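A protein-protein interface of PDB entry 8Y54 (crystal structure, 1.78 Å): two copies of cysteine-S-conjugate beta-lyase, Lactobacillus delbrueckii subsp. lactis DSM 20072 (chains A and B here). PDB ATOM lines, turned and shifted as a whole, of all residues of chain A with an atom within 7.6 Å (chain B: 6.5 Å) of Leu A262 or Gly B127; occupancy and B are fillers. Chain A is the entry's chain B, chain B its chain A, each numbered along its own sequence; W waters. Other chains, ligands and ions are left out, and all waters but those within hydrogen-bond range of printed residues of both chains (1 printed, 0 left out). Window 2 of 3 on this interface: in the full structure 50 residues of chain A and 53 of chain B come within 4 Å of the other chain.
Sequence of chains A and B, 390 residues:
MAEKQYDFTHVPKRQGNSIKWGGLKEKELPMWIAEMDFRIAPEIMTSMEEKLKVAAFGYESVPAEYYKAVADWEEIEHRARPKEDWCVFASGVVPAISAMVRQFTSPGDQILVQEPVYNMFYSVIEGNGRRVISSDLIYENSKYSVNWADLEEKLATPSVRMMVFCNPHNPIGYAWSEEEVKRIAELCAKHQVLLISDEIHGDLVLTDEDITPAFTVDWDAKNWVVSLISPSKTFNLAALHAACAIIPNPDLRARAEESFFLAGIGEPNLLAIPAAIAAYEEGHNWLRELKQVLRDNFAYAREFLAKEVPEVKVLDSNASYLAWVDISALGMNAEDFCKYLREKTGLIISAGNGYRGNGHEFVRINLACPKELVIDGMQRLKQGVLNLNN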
ATOM      1  N   ALA A  99      21.805  35.377 -10.378  1.00  0.00           N
ATOM      2  CA  ALA A  99      20.750  34.369 -10.462  1.00  0.00           C
ATOM      3  C   ALA A  99      19.397  35.011 -10.730  1.00  0.00           C
ATOM      4  O   ALA A  99      18.555  34.448 -11.450  1.00  0.00           O
ATOM      5  CB  ALA A  99      20.703  33.539  -9.174  1.00  0.00           C
ATOM      6  N   ARG A 102      18.955  35.992 -14.350  1.00  0.00           N
ATOM      7  CA  ARG A 102      18.551  34.870 -15.189  1.00  0.00           C
ATOM      8  C   ARG A 102      17.106  34.475 -14.914  1.00  0.00           C
ATOM      9  O   ARG A 102      16.366  34.121 -15.837  1.00  0.00           O
ATOM     10  CB  ARG A 102      19.487  33.676 -14.967  1.00  0.00           C
ATOM     11  CG  ARG A 102      20.880  33.849 -15.580  1.00  0.00           C
ATOM     12  CD  ARG A 102      21.690  32.545 -15.558  1.00  0.00           C
ATOM     13  NE  ARG A 102      21.739  31.993 -14.219  1.00  0.00           N
ATOM     14  CZ  ARG A 102      22.608  32.380 -13.288  1.00  0.00           C
ATOM     15  NH1 ARG A 102      23.534  33.298 -13.568  1.00  0.00           N
ATOM     16  NH2 ARG A 102      22.559  31.837 -12.079  1.00  0.00           N
ATOM     17  N   GLN A 103      16.679  34.546 -13.656  1.00  0.00           N
ATOM     18  CA  GLN A 103      15.368  34.014 -13.302  1.00  0.00           C
ATOM     19  C   GLN A 103      14.245  34.987 -13.637  1.00  0.00           C
ATOM     20  O   GLN A 103      13.153  34.562 -14.046  1.00  0.00           O
ATOM     21  CB  GLN A 103      15.321  33.658 -11.813  1.00  0.00           C
ATOM     22  CG  GLN A 103      14.001  33.030 -11.363  1.00  0.00           C
ATOM     23  CD  GLN A 103      13.796  31.595 -11.857  1.00  0.00           C
ATOM     24  OE1 GLN A 103      13.784  31.337 -13.054  1.00  0.00           O
ATOM     25  NE2 GLN A 103      13.592  30.667 -10.923  1.00  0.00           N
ATOM     26  N   ALA A 256      13.203  33.025  -6.401  1.00  0.00           N
ATOM     27  CA  ALA A 256      14.608  33.406  -6.207  1.00  0.00           C
ATOM     28  C   ALA A 256      15.340  32.250  -5.521  1.00  0.00           C
ATOM     29  O   ALA A 256      16.397  31.863  -5.967  1.00  0.00           O
ATOM     30  CB  ALA A 256      14.666  34.661  -5.385  1.00  0.00           C
ATOM     31  N   GLU A 257      14.744  31.740  -4.454  1.00  0.00           N
ATOM     32  CA  GLU A 257      15.402  30.661  -3.731  1.00  0.00           C
ATOM     33  C   GLU A 257      15.611  29.448  -4.622  1.00  0.00           C
ATOM     34  O   GLU A 257      16.663  28.796  -4.562  1.00  0.00           O
ATOM     35  CB  GLU A 257      14.581  30.276  -2.504  1.00  0.00           C
ATOM     36  CG  GLU A 257      15.080  29.035  -1.812  1.00  0.00           C
ATOM     37  CD  GLU A 257      14.105  28.535  -0.767  1.00  0.00           C
ATOM     38  OE1 GLU A 257      14.563  28.111   0.309  1.00  0.00           O
ATOM     39  OE2 GLU A 257      12.886  28.574  -1.023  1.00  0.00           O
ATOM     40  N   GLU A 258      14.606  29.108  -5.435  1.00  0.00           N
ATOM     41  CA  GLU A 258      14.786  28.020  -6.386  1.00  0.00           C
ATOM     42  C   GLU A 258      15.936  28.321  -7.335  1.00  0.00           C
ATOM     43  O   GLU A 258      16.746  27.439  -7.638  1.00  0.00           O
ATOM     44  CB  GLU A 258      13.491  27.777  -7.164  1.00  0.00           C
ATOM     45  CG  GLU A 258      13.566  26.634  -8.150  1.00  0.00           C
ATOM     46  CD  GLU A 258      12.286  25.819  -8.192  1.00  0.00           C
ATOM     47  OE1 GLU A 258      12.286  24.757  -8.849  1.00  0.00           O
ATOM     48  OE2 GLU A 258      11.283  26.244  -7.566  1.00  0.00           O
ATOM     49  N   SER A 259      16.042  29.575  -7.789  1.00  0.00           N
ATOM     50  CA  SER A 259      17.150  29.935  -8.669  1.00  0.00           C
ATOM     51  C   SER A 259      18.494  29.816  -7.955  1.00  0.00           C
ATOM     52  O   SER A 259      19.477  29.365  -8.555  1.00  0.00           O
ATOM     53  CB  SER A 259      16.959  31.348  -9.205  1.00  0.00           C
ATOM     54  OG  SER A 259      17.889  31.622 -10.238  1.00  0.00           O
ATOM     55  N   PHE A 260      18.561  30.209  -6.678  1.00  0.00           N
ATOM     56  CA  PHE A 260      19.806  30.043  -5.924  1.00  0.00           C
ATOM     57  C   PHE A 260      20.214  28.577  -5.864  1.00  0.00           C
ATOM     58  O   PHE A 260      21.391  28.232  -6.037  1.00  0.00           O
ATOM     59  CB  PHE A 260      19.668  30.596  -4.489  1.00  0.00           C
ATOM     60  CG  PHE A 260      19.338  32.070  -4.404  1.00  0.00           C
ATOM     61  CD1 PHE A 260      19.493  32.906  -5.491  1.00  0.00           C
ATOM     62  CD2 PHE A 260      18.848  32.611  -3.211  1.00  0.00           C
ATOM     63  CE1 PHE A 260      19.158  34.257  -5.410  1.00  0.00           C
ATOM     64  CE2 PHE A 260      18.521  33.947  -3.118  1.00  0.00           C
ATOM     65  CZ  PHE A 260      18.673  34.780  -4.220  1.00  0.00           C
ATOM     66  N   PHE A 261      19.256  27.693  -5.581  1.00  0.00           N
ATOM     67  CA  PHE A 261      19.600  26.286  -5.444  1.00  0.00           C
ATOM     68  C   PHE A 261      20.097  25.713  -6.757  1.00  0.00           C
ATOM     69  O   PHE A 261      21.110  25.003  -6.784  1.00  0.00           O
ATOM     70  CB  PHE A 261      18.402  25.507  -4.921  1.00  0.00           C
ATOM     71  CG  PHE A 261      18.343  25.503  -3.443  1.00  0.00           C
ATOM     72  CD1 PHE A 261      19.188  24.683  -2.714  1.00  0.00           C
ATOM     73  CD2 PHE A 261      17.520  26.389  -2.772  1.00  0.00           C
ATOM     74  CE1 PHE A 261      19.166  24.706  -1.342  1.00  0.00           C
ATOM     75  CE2 PHE A 261      17.492  26.415  -1.409  1.00  0.00           C
ATOM     76  CZ  PHE A 261      18.315  25.567  -0.688  1.00  0.00           C
ATOM     77  N   LEU A 262      19.399  26.035  -7.854  1.00  0.00           N
ATOM     78  CA  LEU A 262      19.759  25.551  -9.181  1.00  0.00           C
ATOM     79  C   LEU A 262      21.153  26.012  -9.580  1.00  0.00           C
ATOM     80  O   LEU A 262      21.903  25.267 -10.219  1.00  0.00           O
ATOM     81  CB  LEU A 262      18.734  26.051 -10.206  1.00  0.00           C
ATOM     82  CG  LEU A 262      17.828  25.070 -10.941  1.00  0.00           C
ATOM     83  CD1 LEU A 262      17.260  25.732 -12.205  1.00  0.00           C
ATOM     84  CD2 LEU A 262      18.590  23.800 -11.283  1.00  0.00           C
ATOM     85  N   ALA A 263      21.510  27.245  -9.223  1.00  0.00           N
ATOM     86  CA  ALA A 263      22.808  27.809  -9.582  1.00  0.00           C
ATOM     87  C   ALA A 263      23.952  27.257  -8.734  1.00  0.00           C
ATOM     88  O   ALA A 263      25.118  27.344  -9.145  1.00  0.00           O
ATOM     89  CB  ALA A 263      22.764  29.327  -9.436  1.00  0.00           C
ATOM     90  N   GLY A 264      23.653  26.712  -7.559  1.00  0.00           N
ATOM     91  CA  GLY A 264      24.694  26.299  -6.641  1.00  0.00           C
ATOM     92  C   GLY A 264      25.067  27.311  -5.581  1.00  0.00           C
ATOM     93  O   GLY A 264      26.187  27.252  -5.051  1.00  0.00           O
ATOM     94  N   ILE A 265      24.178  28.248  -5.252  1.00  0.00           N
ATOM     95  CA  ILE A 265      24.521  29.294  -4.286  1.00  0.00           C
ATOM     96  C   ILE A 265      23.455  29.345  -3.196  1.00  0.00           C
ATOM     97  O   ILE A 265      23.361  30.327  -2.451  1.00  0.00           O
ATOM     98  CB  ILE A 265      24.677  30.663  -4.975  1.00  0.00           C
ATOM     99  CG1 ILE A 265      23.387  31.038  -5.727  1.00  0.00           C
ATOM    100  CG2 ILE A 265      25.853  30.654  -5.957  1.00  0.00           C
ATOM    101  CD1 ILE A 265      23.263  32.550  -6.013  1.00  0.00           C
ATOM    102  N   GLY A 266      22.649  28.293  -3.089  1.00  0.00           N
ATOM    103  CA  GLY A 266      21.615  28.257  -2.069  1.00  0.00           C
ATOM    104  C   GLY A 266      21.975  27.505  -0.796  1.00  0.00           C
ATOM    105  O   GLY A 266      21.221  27.563   0.181  1.00  0.00           O
ATOM    106  N   VAL B  94      27.951  19.488  -8.921  1.00  0.00           N
ATOM    107  CA  VAL B  94      26.569  19.624  -9.443  1.00  0.00           C
ATOM    108  C   VAL B  94      26.341  21.040  -9.980  1.00  0.00           C
ATOM    109  O   VAL B  94      25.865  21.160 -11.103  1.00  0.00           O
ATOM    110  CB  VAL B  94      25.517  19.117  -8.444  1.00  0.00           C
ATOM    111  CG1 VAL B  94      24.106  19.514  -8.819  1.00  0.00           C
ATOM    112  CG2 VAL B  94      25.621  17.615  -8.253  1.00  0.00           C
ATOM    113  N   PRO B  95      26.696  22.118  -9.255  1.00  0.00           N
ATOM    114  CA  PRO B  95      26.583  23.451  -9.830  1.00  0.00           C
ATOM    115  C   PRO B  95      27.404  23.641 -11.120  1.00  0.00           C
ATOM    116  O   PRO B  95      27.011  24.394 -11.948  1.00  0.00           O
ATOM    117  CB  PRO B  95      27.075  24.384  -8.717  1.00  0.00           C
ATOM    118  CG  PRO B  95      26.886  23.615  -7.444  1.00  0.00           C
ATOM    119  CD  PRO B  95      27.055  22.170  -7.833  1.00  0.00           C
ATOM    120  N   SER B  98      25.253  22.161 -13.790  1.00  0.00           N
ATOM    121  CA  SER B  98      24.198  23.134 -14.042  1.00  0.00           C
ATOM    122  C   SER B  98      24.681  24.254 -14.958  1.00  0.00           C
ATOM    123  O   SER B  98      24.023  24.584 -15.950  1.00  0.00           O
ATOM    124  CB  SER B  98      23.687  23.693 -12.713  1.00  0.00           C
ATOM    125  OG  SER B  98      22.494  24.428 -12.870  1.00  0.00           O
ATOM    126  N   ALA B  99      25.830  24.853 -14.646  1.00  0.00           N
ATOM    127  CA  ALA B  99      26.317  25.968 -15.454  1.00  0.00           C
ATOM    128  C   ALA B  99      26.650  25.525 -16.871  1.00  0.00           C
ATOM    129  O   ALA B  99      26.409  26.263 -17.833  1.00  0.00           O
ATOM    130  CB  ALA B  99      27.546  26.613 -14.795  1.00  0.00           C
ATOM    131  N   ARG B 102      23.623  25.187 -19.027  1.00  0.00           N
ATOM    132  CA  ARG B 102      23.149  26.462 -19.555  1.00  0.00           C
ATOM    133  C   ARG B 102      24.050  27.009 -20.651  1.00  0.00           C
ATOM    134  O   ARG B 102      23.565  27.677 -21.575  1.00  0.00           O
ATOM    135  CB  ARG B 102      23.034  27.483 -18.431  1.00  0.00           C
ATOM    136  CG  ARG B 102      21.911  27.182 -17.474  1.00  0.00           C
ATOM    137  CD  ARG B 102      21.683  28.386 -16.567  1.00  0.00           C
ATOM    138  NE  ARG B 102      22.859  28.688 -15.746  1.00  0.00           N
ATOM    139  CZ  ARG B 102      23.152  28.058 -14.609  1.00  0.00           C
ATOM    140  NH1 ARG B 102      22.352  27.092 -14.147  1.00  0.00           N
ATOM    141  NH2 ARG B 102      24.241  28.385 -13.934  1.00  0.00           N
ATOM    142  N   TYR B 122      18.978  14.654 -12.977  1.00  0.00           N
ATOM    143  CA  TYR B 122      17.665  15.062 -13.466  1.00  0.00           C
ATOM    144  C   TYR B 122      17.318  16.468 -13.004  1.00  0.00           C
ATOM    145  O   TYR B 122      16.745  17.256 -13.765  1.00  0.00           O
ATOM    146  CB  TYR B 122      16.587  14.087 -13.002  1.00  0.00           C
ATOM    147  CG  TYR B 122      16.974  12.649 -13.181  1.00  0.00           C
ATOM    148  CD1 TYR B 122      17.294  12.148 -14.437  1.00  0.00           C
ATOM    149  CD2 TYR B 122      17.011  11.789 -12.100  1.00  0.00           C
ATOM    150  CE1 TYR B 122      17.654  10.821 -14.602  1.00  0.00           C
ATOM    151  CE2 TYR B 122      17.374  10.460 -12.252  1.00  0.00           C
ATOM    152  CZ  TYR B 122      17.684   9.981 -13.503  1.00  0.00           C
ATOM    153  OH  TYR B 122      18.037   8.662 -13.638  1.00  0.00           O
ATOM    154  N   SER B 123      17.643  16.793 -11.757  1.00  0.00           N
ATOM    155  CA  SER B 123      17.288  18.104 -11.233  1.00  0.00           C
ATOM    156  C   SER B 123      17.989  19.219 -12.001  1.00  0.00           C
ATOM    157  O   SER B 123      17.384  20.265 -12.272  1.00  0.00           O
ATOM    158  CB  SER B 123      17.616  18.169  -9.730  1.00  0.00           C
ATOM    159  OG  SER B 123      17.804  19.509  -9.316  1.00  0.00           O
ATOM    160  N   VAL B 124      19.260  19.028 -12.366  1.00  0.00           N
ATOM    161  CA  VAL B 124      19.947  20.115 -13.060  1.00  0.00           C
ATOM    162  C   VAL B 124      19.598  20.151 -14.538  1.00  0.00           C
ATOM    163  O   VAL B 124      19.639  21.220 -15.148  1.00  0.00           O
ATOM    164  CB  VAL B 124      21.475  20.065 -12.879  1.00  0.00           C
ATOM    165  CG1 VAL B 124      21.823  20.121 -11.404  1.00  0.00           C
ATOM    166  CG2 VAL B 124      22.084  18.848 -13.576  1.00  0.00           C
ATOM    167  N   ILE B 125      19.297  19.007 -15.151  1.00  0.00           N
ATOM    168  CA  ILE B 125      18.883  19.004 -16.554  1.00  0.00           C
ATOM    169  C   ILE B 125      17.480  19.583 -16.684  1.00  0.00           C
ATOM    170  O   ILE B 125      17.246  20.568 -17.402  1.00  0.00           O
ATOM    171  CB  ILE B 125      18.958  17.577 -17.126  1.00  0.00           C
ATOM    172  CG1 ILE B 125      20.416  17.122 -17.185  1.00  0.00           C
ATOM    173  CG2 ILE B 125      18.314  17.498 -18.517  1.00  0.00           C
ATOM    174  CD1 ILE B 125      20.585  15.666 -17.521  1.00  0.00           C
ATOM    175  N   GLU B 126      16.530  18.986 -15.971  1.00  0.00           N
ATOM    176  CA  GLU B 126      15.139  19.420 -16.066  1.00  0.00           C
ATOM    177  C   GLU B 126      14.930  20.785 -15.423  1.00  0.00           C
ATOM    178  O   GLU B 126      14.173  21.610 -15.946  1.00  0.00           O
ATOM    179  CB  GLU B 126      14.230  18.363 -15.434  1.00  0.00           C
ATOM    180  CG  GLU B 126      14.249  17.048 -16.206  1.00  0.00           C
ATOM    181  CD  GLU B 126      13.513  15.929 -15.514  1.00  0.00           C
ATOM    182  OE1 GLU B 126      13.250  14.891 -16.162  1.00  0.00           O
ATOM    183  OE2 GLU B 126      13.189  16.080 -14.321  1.00  0.00           O
ATOM    184  N   GLY B 127      15.594  21.050 -14.298  1.00  0.00           N
ATOM    185  CA  GLY B 127      15.450  22.349 -13.661  1.00  0.00           C
ATOM    186  C   GLY B 127      15.872  23.494 -14.552  1.00  0.00           C
ATOM    187  O   GLY B 127      15.358  24.611 -14.418  1.00  0.00           O
ATOM    188  N   ASN B 128      16.826  23.242 -15.456  1.00  0.00           N
ATOM    189  CA  ASN B 128      17.271  24.251 -16.406  1.00  0.00           C
ATOM    190  C   ASN B 128      16.502  24.202 -17.711  1.00  0.00           C
ATOM    191  O   ASN B 128      16.863  24.923 -18.643  1.00  0.00           O
ATOM    192  CB  ASN B 128      18.762  24.097 -16.717  1.00  0.00           C
ATOM    193  CG  ASN B 128      19.648  24.652 -15.615  1.00  0.00           C
ATOM    194  OD1 ASN B 128      19.576  25.830 -15.283  1.00  0.00           O
ATOM    195  ND2 ASN B 128      20.483  23.803 -15.044  1.00  0.00           N
ATOM    196  N   GLY B 129      15.494  23.346 -17.815  1.00  0.00           N
ATOM    197  CA  GLY B 129      14.680  23.343 -19.014  1.00  0.00           C
ATOM    198  C   GLY B 129      15.280  22.577 -20.166  1.00  0.00           C
ATOM    199  O   GLY B 129      14.956  22.848 -21.329  1.00  0.00           O
ATOM    200  N   ARG B 130      16.152  21.625 -19.876  1.00  0.00           N
ATOM    201  CA  ARG B 130      16.577  20.652 -20.862  1.00  0.00           C
ATOM    202  C   ARG B 130      15.847  19.347 -20.579  1.00  0.00           C
ATOM    203  O   ARG B 130      15.183  19.199 -19.550  1.00  0.00           O
ATOM    204  CB  ARG B 130      18.097  20.484 -20.858  1.00  0.00           C
ATOM    205  CG  ARG B 130      18.840  21.545 -21.669  1.00  0.00           C
ATOM    206  CD  ARG B 130      18.724  22.955 -21.061  1.00  0.00           C
ATOM    207  NE  ARG B 130      19.629  23.943 -21.657  1.00  0.00           N
ATOM    208  CZ  ARG B 130      19.633  25.234 -21.328  1.00  0.00           C
ATOM    209  NH1 ARG B 130      18.771  25.679 -20.430  1.00  0.00           N
ATOM    210  NH2 ARG B 130      20.491  26.085 -21.894  1.00  0.00           N
HETATM  211  O   HOH W   1      25.259  26.644 -11.873  1.00  0.00           O
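Water W1 lies within hydrogen-bond range of O of Ala A263 (2.8 Å), O of Pro B95 (2.9 Å), NH2 of Arg B102 (2.9 Å) and N of Ala B99 (3.4 Å).
The side-chain hydroxyl of Ser B98 sits at hydrogen-bond distance from the guanidinium group of Arg B102, at 3.0 Å.
The side-chain amide nitrogen (ND2) of Asn B128 lies within hydrogen-bond range of the side-chain hydroxyl (OG) of Ser B98, at 3.0 Å.
The guanidinium group of Arg B102 sits at hydrogen-bond distance from the side-chain amide oxygen of Asn B128 (3.3 Å).
O of Arg B102 sits at hydrogen-bond distance from NH2 of Arg B130 (3.5 Å).
The backbone carbonyl oxygen of Val B124 sits at hydrogen-bond distance from the side-chain amide nitrogen of Asn B128 (2.7 Å).
NH1 of Arg B130 sits at hydrogen-bond distance from O of Asn B128 (2.7 Å).
Among the printed residues, pairs that only touch across the chains: Leu A262 with Gly B127 (3.1 Å), Gly A264 with Pro B95 (3.6 Å), Ala A263 with Pro B95 (3.6 Å), Arg A102 with Arg B102 (3.8 Å), Leu A262 with Asn B128 (3.9 Å) and Leu A262 with Ser B123 (3.9 Å).
Leu A262 touches just these residues of chain B: Ser B98, Ser B123, Gly B127 and Asn B128.
Gly B127 touches one residue of chain A.
Printed residues of chain A within 4 Å of Ser B123: Leu A262.
Printed residues of chain B within 4 Å of Ala A263: Pro B95.
Of the printed residues of chain A, Arg B102 touches Arg A102 (3.8 Å).
Printed residues of chain A within 4 Å of Asn B128: Leu A262.
Tyr B122 touches none of the printed residues of chain A.
The nearest residue of chain B that does not touch Leu A262 is Val B124 (4.3 Å).
The nearest printed residue of chain B that does not touch Gly A264 is Ser B98 (5.9 Å).
OG of Ser B98 sits at hydrogen-bond distance from O of Leu A262 (2.8 Å).
Of the 14 printed residues of chain B, 6 touch a printed residue of chain A.
Hydrophobic or aromatic side chains of chain B that line the printed part of chain A: Pro B95.
Of the 14 printed residues of chain A, 4 touch a printed residue of chain B.
Printed residues of chain A that touch a printed residue of chain B: Arg A102, Leu A262, Ala A263 and Gly A264.
Hydrophobic or aromatic side chains of chain A within 4 Å of the printed part of chain B: Leu A262.
Arg B102 touches its own counterpart, Arg A102.
Positions printed for both chains: 99 and 102.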
